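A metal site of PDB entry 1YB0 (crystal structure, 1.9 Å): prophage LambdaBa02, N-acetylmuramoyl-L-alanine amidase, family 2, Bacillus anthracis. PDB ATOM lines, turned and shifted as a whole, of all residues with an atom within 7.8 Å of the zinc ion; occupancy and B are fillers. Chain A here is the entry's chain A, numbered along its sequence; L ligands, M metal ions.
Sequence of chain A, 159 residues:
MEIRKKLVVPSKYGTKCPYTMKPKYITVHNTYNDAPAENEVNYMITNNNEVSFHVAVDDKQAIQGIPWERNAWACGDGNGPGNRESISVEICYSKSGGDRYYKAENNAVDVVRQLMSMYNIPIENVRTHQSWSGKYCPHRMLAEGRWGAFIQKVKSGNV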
ATOM      1  N   THR A  27     -14.510 -15.004  -9.738  1.00  0.00           N
ATOM      2  CA  THR A  27     -13.278 -15.267  -8.988  1.00  0.00           C
ATOM      3  C   THR A  27     -12.428 -14.014  -8.964  1.00  0.00           C
ATOM      4  O   THR A  27     -12.126 -13.465 -10.015  1.00  0.00           O
ATOM      5  CB  THR A  27     -12.443 -16.377  -9.650  1.00  0.00           C
ATOM      6  OG1 THR A  27     -13.219 -17.584  -9.736  1.00  0.00           O
ATOM      7  CG2 THR A  27     -11.167 -16.623  -8.840  1.00  0.00           C
ATOM      8  N   VAL A  28     -12.070 -13.568  -7.760  1.00  0.00           N
ATOM      9  CA  VAL A  28     -11.268 -12.362  -7.590  1.00  0.00           C
ATOM     10  C   VAL A  28      -9.796 -12.720  -7.373  1.00  0.00           C
ATOM     11  O   VAL A  28      -9.459 -13.633  -6.603  1.00  0.00           O
ATOM     12  CB  VAL A  28     -11.790 -11.528  -6.389  1.00  0.00           C
ATOM     13  CG1 VAL A  28     -10.948 -10.282  -6.202  1.00  0.00           C
ATOM     14  CG2 VAL A  28     -13.240 -11.173  -6.628  1.00  0.00           C
ATOM     15  N   HIS A  29      -8.934 -11.991  -8.081  1.00  0.00           N
ATOM     16  CA  HIS A  29      -7.491 -12.195  -8.046  1.00  0.00           C
ATOM     17  C   HIS A  29      -6.764 -10.885  -7.768  1.00  0.00           C
ATOM     18  O   HIS A  29      -7.347  -9.812  -7.846  1.00  0.00           O
ATOM     19  CB  HIS A  29      -6.975 -12.683  -9.415  1.00  0.00           C
ATOM     20  CG  HIS A  29      -7.672 -13.886  -9.977  1.00  0.00           C
ATOM     21  ND1 HIS A  29      -7.122 -15.152  -9.947  1.00  0.00           N
ATOM     22  CD2 HIS A  29      -8.801 -13.992 -10.714  1.00  0.00           C
ATOM     23  CE1 HIS A  29      -7.870 -15.977 -10.652  1.00  0.00           C
ATOM     24  NE2 HIS A  29      -8.896 -15.297 -11.126  1.00  0.00           N
ATOM     25  N   ASN A  30      -5.480 -10.997  -7.434  1.00  0.00           N
ATOM     26  CA  ASN A  30      -4.587  -9.846  -7.237  1.00  0.00           C
ATOM     27  C   ASN A  30      -3.510 -10.183  -8.269  1.00  0.00           C
ATOM     28  O   ASN A  30      -3.120 -11.338  -8.372  1.00  0.00           O
ATOM     29  CB  ASN A  30      -3.978  -9.820  -5.818  1.00  0.00           C
ATOM     30  CG  ASN A  30      -4.832  -9.050  -4.812  1.00  0.00           C
ATOM     31  OD1 ASN A  30      -4.479  -8.958  -3.636  1.00  0.00           O
ATOM     32  ND2 ASN A  30      -5.951  -8.488  -5.266  1.00  0.00           N
ATOM     33  N   THR A  31      -3.039  -9.224  -9.047  1.00  0.00           N
ATOM     34  CA  THR A  31      -2.028  -9.519 -10.065  1.00  0.00           C
ATOM     35  C   THR A  31      -0.626  -9.791  -9.521  1.00  0.00           C
ATOM     36  O   THR A  31       0.190 -10.418 -10.193  1.00  0.00           O
ATOM     37  CB  THR A  31      -1.869  -8.369 -11.062  1.00  0.00           C
ATOM     38  OG1 THR A  31      -1.388  -7.204 -10.358  1.00  0.00           O
ATOM     39  CG2 THR A  31      -3.199  -8.026 -11.729  1.00  0.00           C
ATOM     40  N   ALA A  74      -7.447 -19.180 -15.484  1.00  0.00           N
ATOM     41  CA  ALA A  74      -6.888 -18.375 -14.414  1.00  0.00           C
ATOM     42  C   ALA A  74      -6.997 -18.935 -13.022  1.00  0.00           C
ATOM     43  O   ALA A  74      -6.346 -18.409 -12.118  1.00  0.00           O
ATOM     44  CB  ALA A  74      -7.542 -17.007 -14.446  1.00  0.00           C
ATOM     45  N   CYS A  75      -7.797 -19.989 -12.831  1.00  0.00           N
ATOM     46  CA  CYS A  75      -8.045 -20.545 -11.495  1.00  0.00           C
ATOM     47  C   CYS A  75      -7.220 -21.742 -11.050  1.00  0.00           C
ATOM     48  O   CYS A  75      -7.375 -22.213  -9.916  1.00  0.00           O
ATOM     49  CB  CYS A  75      -9.535 -20.873 -11.363  1.00  0.00           C
ATOM     50  SG  CYS A  75     -10.605 -19.432 -11.630  1.00  0.00           S
ATOM     51  N   GLY A  76      -6.382 -22.252 -11.942  1.00  0.00           N
ATOM     52  CA  GLY A  76      -5.526 -23.376 -11.629  1.00  0.00           C
ATOM     53  C   GLY A  76      -6.161 -24.739 -11.368  1.00  0.00           C
ATOM     54  O   GLY A  76      -5.495 -25.625 -10.845  1.00  0.00           O
ATOM     55  N   SER A  88     -13.140 -14.383 -14.141  1.00  0.00           N
ATOM     56  CA  SER A  88     -12.015 -13.899 -13.350  1.00  0.00           C
ATOM     57  C   SER A  88     -11.732 -12.418 -13.458  1.00  0.00           C
ATOM     58  O   SER A  88     -11.611 -11.880 -14.559  1.00  0.00           O
ATOM     59  CB  SER A  88     -10.748 -14.683 -13.723  1.00  0.00           C
ATOM     60  OG  SER A  88     -10.641 -15.875 -12.955  1.00  0.00           O
ATOM     61  N   VAL A  89     -11.629 -11.761 -12.295  1.00  0.00           N
ATOM     62  CA  VAL A  89     -11.343 -10.342 -12.172  1.00  0.00           C
ATOM     63  C   VAL A  89      -9.978 -10.194 -11.522  1.00  0.00           C
ATOM     64  O   VAL A  89      -9.754 -10.704 -10.426  1.00  0.00           O
ATOM     65  CB  VAL A  89     -12.373  -9.644 -11.238  1.00  0.00           C
ATOM     66  CG1 VAL A  89     -12.033  -8.147 -11.110  1.00  0.00           C
ATOM     67  CG2 VAL A  89     -13.795  -9.823 -11.792  1.00  0.00           C
ATOM     68  N   GLU A  90      -9.057  -9.508 -12.198  1.00  0.00           N
ATOM     69  CA  GLU A  90      -7.709  -9.285 -11.683  1.00  0.00           C
ATOM     70  C   GLU A  90      -7.629  -7.842 -11.195  1.00  0.00           C
ATOM     71  O   GLU A  90      -7.944  -6.908 -11.924  1.00  0.00           O
ATOM     72  CB  GLU A  90      -6.685  -9.498 -12.803  1.00  0.00           C
ATOM     73  CG  GLU A  90      -6.504 -10.930 -13.281  1.00  0.00           C
ATOM     74  CD  GLU A  90      -5.486 -11.696 -12.441  1.00  0.00           C
ATOM     75  OE1 GLU A  90      -4.877 -11.088 -11.555  1.00  0.00           O
ATOM     76  OE2 GLU A  90      -5.304 -12.904 -12.686  1.00  0.00           O
ATOM     77  N   THR A 128     -12.446 -16.631  -4.164  1.00  0.00           N
ATOM     78  CA  THR A 128     -11.022 -16.304  -4.290  1.00  0.00           C
ATOM     79  C   THR A 128     -10.408 -17.387  -5.180  1.00  0.00           C
ATOM     80  O   THR A 128     -10.938 -18.484  -5.288  1.00  0.00           O
ATOM     81  CB  THR A 128     -10.288 -16.397  -2.935  1.00  0.00           C
ATOM     82  OG1 THR A 128     -10.463 -17.717  -2.404  1.00  0.00           O
ATOM     83  CG2 THR A 128     -10.813 -15.375  -1.943  1.00  0.00           C
ATOM     84  N   HIS A 129      -9.288 -17.061  -5.816  1.00  0.00           N
ATOM     85  CA  HIS A 129      -8.569 -18.026  -6.649  1.00  0.00           C
ATOM     86  C   HIS A 129      -8.161 -19.134  -5.673  1.00  0.00           C
ATOM     87  O   HIS A 129      -8.256 -20.320  -5.988  1.00  0.00           O
ATOM     88  CB  HIS A 129      -7.333 -17.338  -7.266  1.00  0.00           C
ATOM     89  CG  HIS A 129      -6.430 -18.257  -8.036  1.00  0.00           C
ATOM     90  ND1 HIS A 129      -5.383 -17.785  -8.811  1.00  0.00           N
ATOM     91  CD2 HIS A 129      -6.388 -19.610  -8.147  1.00  0.00           C
ATOM     92  CE1 HIS A 129      -4.735 -18.799  -9.358  1.00  0.00           C
ATOM     93  NE2 HIS A 129      -5.333 -19.924  -8.976  1.00  0.00           N
ATOM     94  N   GLN A 130      -7.738 -18.745  -4.469  1.00  0.00           N
ATOM     95  CA  GLN A 130      -7.330 -19.703  -3.449  1.00  0.00           C
ATOM     96  C   GLN A 130      -8.366 -20.811  -3.232  1.00  0.00           C
ATOM     97  O   GLN A 130      -8.012 -21.970  -3.062  1.00  0.00           O
ATOM     98  CB  GLN A 130      -7.053 -18.998  -2.124  1.00  0.00           C
ATOM     99  CG  GLN A 130      -6.654 -19.910  -0.955  1.00  0.00           C
ATOM    100  CD  GLN A 130      -6.583 -19.149   0.347  1.00  0.00           C
ATOM    101  OE1 GLN A 130      -7.557 -18.510   0.757  1.00  0.00           O
ATOM    102  NE2 GLN A 130      -5.445 -19.220   1.030  1.00  0.00           N
ATOM    103  N   SER A 133      -7.832 -23.549  -6.135  1.00  0.00           N
ATOM    104  CA  SER A 133      -6.588 -24.273  -6.322  1.00  0.00           C
ATOM    105  C   SER A 133      -5.648 -24.245  -5.132  1.00  0.00           C
ATOM    106  O   SER A 133      -4.613 -24.910  -5.148  1.00  0.00           O
ATOM    107  CB  SER A 133      -5.842 -23.701  -7.525  1.00  0.00           C
ATOM    108  OG  SER A 133      -5.332 -22.414  -7.185  1.00  0.00           O
ATOM    109  N   LYS A 135      -3.920 -21.707  -4.248  1.00  0.00           N
ATOM    110  CA  LYS A 135      -2.890 -20.678  -4.467  1.00  0.00           C
ATOM    111  C   LYS A 135      -3.232 -19.497  -3.574  1.00  0.00           C
ATOM    112  O   LYS A 135      -4.402 -19.179  -3.370  1.00  0.00           O
ATOM    113  CB  LYS A 135      -2.863 -20.226  -5.938  1.00  0.00           C
ATOM    114  CG  LYS A 135      -1.769 -19.210  -6.249  1.00  0.00           C
ATOM    115  CD  LYS A 135      -1.647 -18.930  -7.725  1.00  0.00           C
ATOM    116  CE  LYS A 135      -0.455 -18.000  -8.002  1.00  0.00           C
ATOM    117  NZ  LYS A 135      -0.416 -17.502  -9.405  1.00  0.00           N
ATOM    118  N   TYR A 136      -2.205 -18.845  -3.038  1.00  0.00           N
ATOM    119  CA  TYR A 136      -2.391 -17.691  -2.161  1.00  0.00           C
ATOM    120  C   TYR A 136      -2.720 -16.456  -3.004  1.00  0.00           C
ATOM    121  O   TYR A 136      -1.884 -15.563  -3.179  1.00  0.00           O
ATOM    122  CB  TYR A 136      -1.130 -17.464  -1.341  1.00  0.00           C
ATOM    123  CG  TYR A 136      -1.291 -16.504  -0.180  1.00  0.00           C
ATOM    124  CD1 TYR A 136      -2.016 -16.870   0.954  1.00  0.00           C
ATOM    125  CD2 TYR A 136      -0.699 -15.242  -0.197  1.00  0.00           C
ATOM    126  CE1 TYR A 136      -2.138 -16.020   2.046  1.00  0.00           C
ATOM    127  CE2 TYR A 136      -0.817 -14.372   0.905  1.00  0.00           C
ATOM    128  CZ  TYR A 136      -1.529 -14.770   2.017  1.00  0.00           C
ATOM    129  OH  TYR A 136      -1.619 -13.951   3.117  1.00  0.00           O
ATOM    130  N   CYS A 137      -3.934 -16.438  -3.548  1.00  0.00           N
ATOM    131  CA  CYS A 137      -4.427 -15.313  -4.369  1.00  0.00           C
ATOM    132  C   CYS A 137      -5.909 -15.168  -4.030  1.00  0.00           C
ATOM    133  O   CYS A 137      -6.638 -16.161  -4.023  1.00  0.00           O
ATOM    134  CB  CYS A 137      -4.278 -15.624  -5.876  1.00  0.00           C
ATOM    135  SG  CYS A 137      -5.052 -14.391  -6.975  1.00  0.00           S
ATOM    136  N   PRO A 138      -6.388 -13.918  -3.847  1.00  0.00           N
ATOM    137  CA  PRO A 138      -5.698 -12.610  -3.925  1.00  0.00           C
ATOM    138  C   PRO A 138      -4.738 -12.352  -2.780  1.00  0.00           C
ATOM    139  O   PRO A 138      -5.150 -12.037  -1.656  1.00  0.00           O
ATOM    140  CB  PRO A 138      -6.862 -11.617  -3.972  1.00  0.00           C
ATOM    141  CG  PRO A 138      -7.912 -12.266  -3.135  1.00  0.00           C
ATOM    142  CD  PRO A 138      -7.825 -13.738  -3.504  1.00  0.00           C
ATOM    143  N   HIS A 139      -3.449 -12.424  -3.080  1.00  0.00           N
ATOM    144  CA  HIS A 139      -2.430 -12.296  -2.053  1.00  0.00           C
ATOM    145  C   HIS A 139      -2.574 -11.133  -1.067  1.00  0.00           C
ATOM    146  O   HIS A 139      -2.585 -11.365   0.132  1.00  0.00           O
ATOM    147  CB  HIS A 139      -1.046 -12.288  -2.690  1.00  0.00           C
ATOM    148  CG  HIS A 139      -0.626 -10.956  -3.219  1.00  0.00           C
ATOM    149  ND1 HIS A 139       0.079 -10.041  -2.454  1.00  0.00           N
ATOM    150  CD2 HIS A 139      -0.842 -10.358  -4.406  1.00  0.00           C
ATOM    151  CE1 HIS A 139       0.277  -8.949  -3.159  1.00  0.00           C
ATOM    152  NE2 HIS A 139      -0.268  -9.115  -4.357  1.00  0.00           N
HETATM  153  P1  LIG L   1      -2.628 -14.979 -10.472  1.00  0.00           P
HETATM  154  O1  LIG L   1      -1.902 -15.741 -11.516  1.00  0.00           O
HETATM  155  O2  LIG L   1      -2.585 -15.722  -9.189  1.00  0.00           O
HETATM  156  O3  LIG L   1      -1.991 -13.635 -10.301  1.00  0.00           O
HETATM  157  O4  LIG L   1      -4.040 -14.801 -10.892  1.00  0.00           O
HETATM  158 ZN    ZN M   1      -5.228 -15.515  -8.983  1.00  0.00          ZN
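Of the 20 residues printed, 3 come within 4 Å of the zinc ion.
NE2 of His 29 sits at hydrogen-bond distance from OG of Ser 88, 2.6 Å away.
The backbone NH (N) of His 29 lies within hydrogen-bond range of the backbone carbonyl oxygen (O) of Val 89 (2.8 Å).
NE2 of His 129 sits at hydrogen-bond distance from O of Cys 75 (3.2 Å).
NE2 of His 129 sits at hydrogen-bond distance from OG of Ser 133 (3.1 Å).
N of Asn 30 sits close to SG of Cys 137 (3.5 Å).
The backbone carbonyl oxygen (O) of Cys 137 is in hydrogen-bond range of the backbone NH (N) of Gln 130 (2.8 Å).
The zinc ion is bound by a ring nitrogen (ND1) of His 29 (2.2 Å), a ring nitrogen (ND1) of His 129 (2.3 Å), the side-chain sulfur (SG) of Cys 137 (2.3 Å) and an oxygen (O4) of the ligand (2.4 Å).
Slightly farther from the zinc ion lies an oxygen (O2) of the ligand (2.7 Å).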
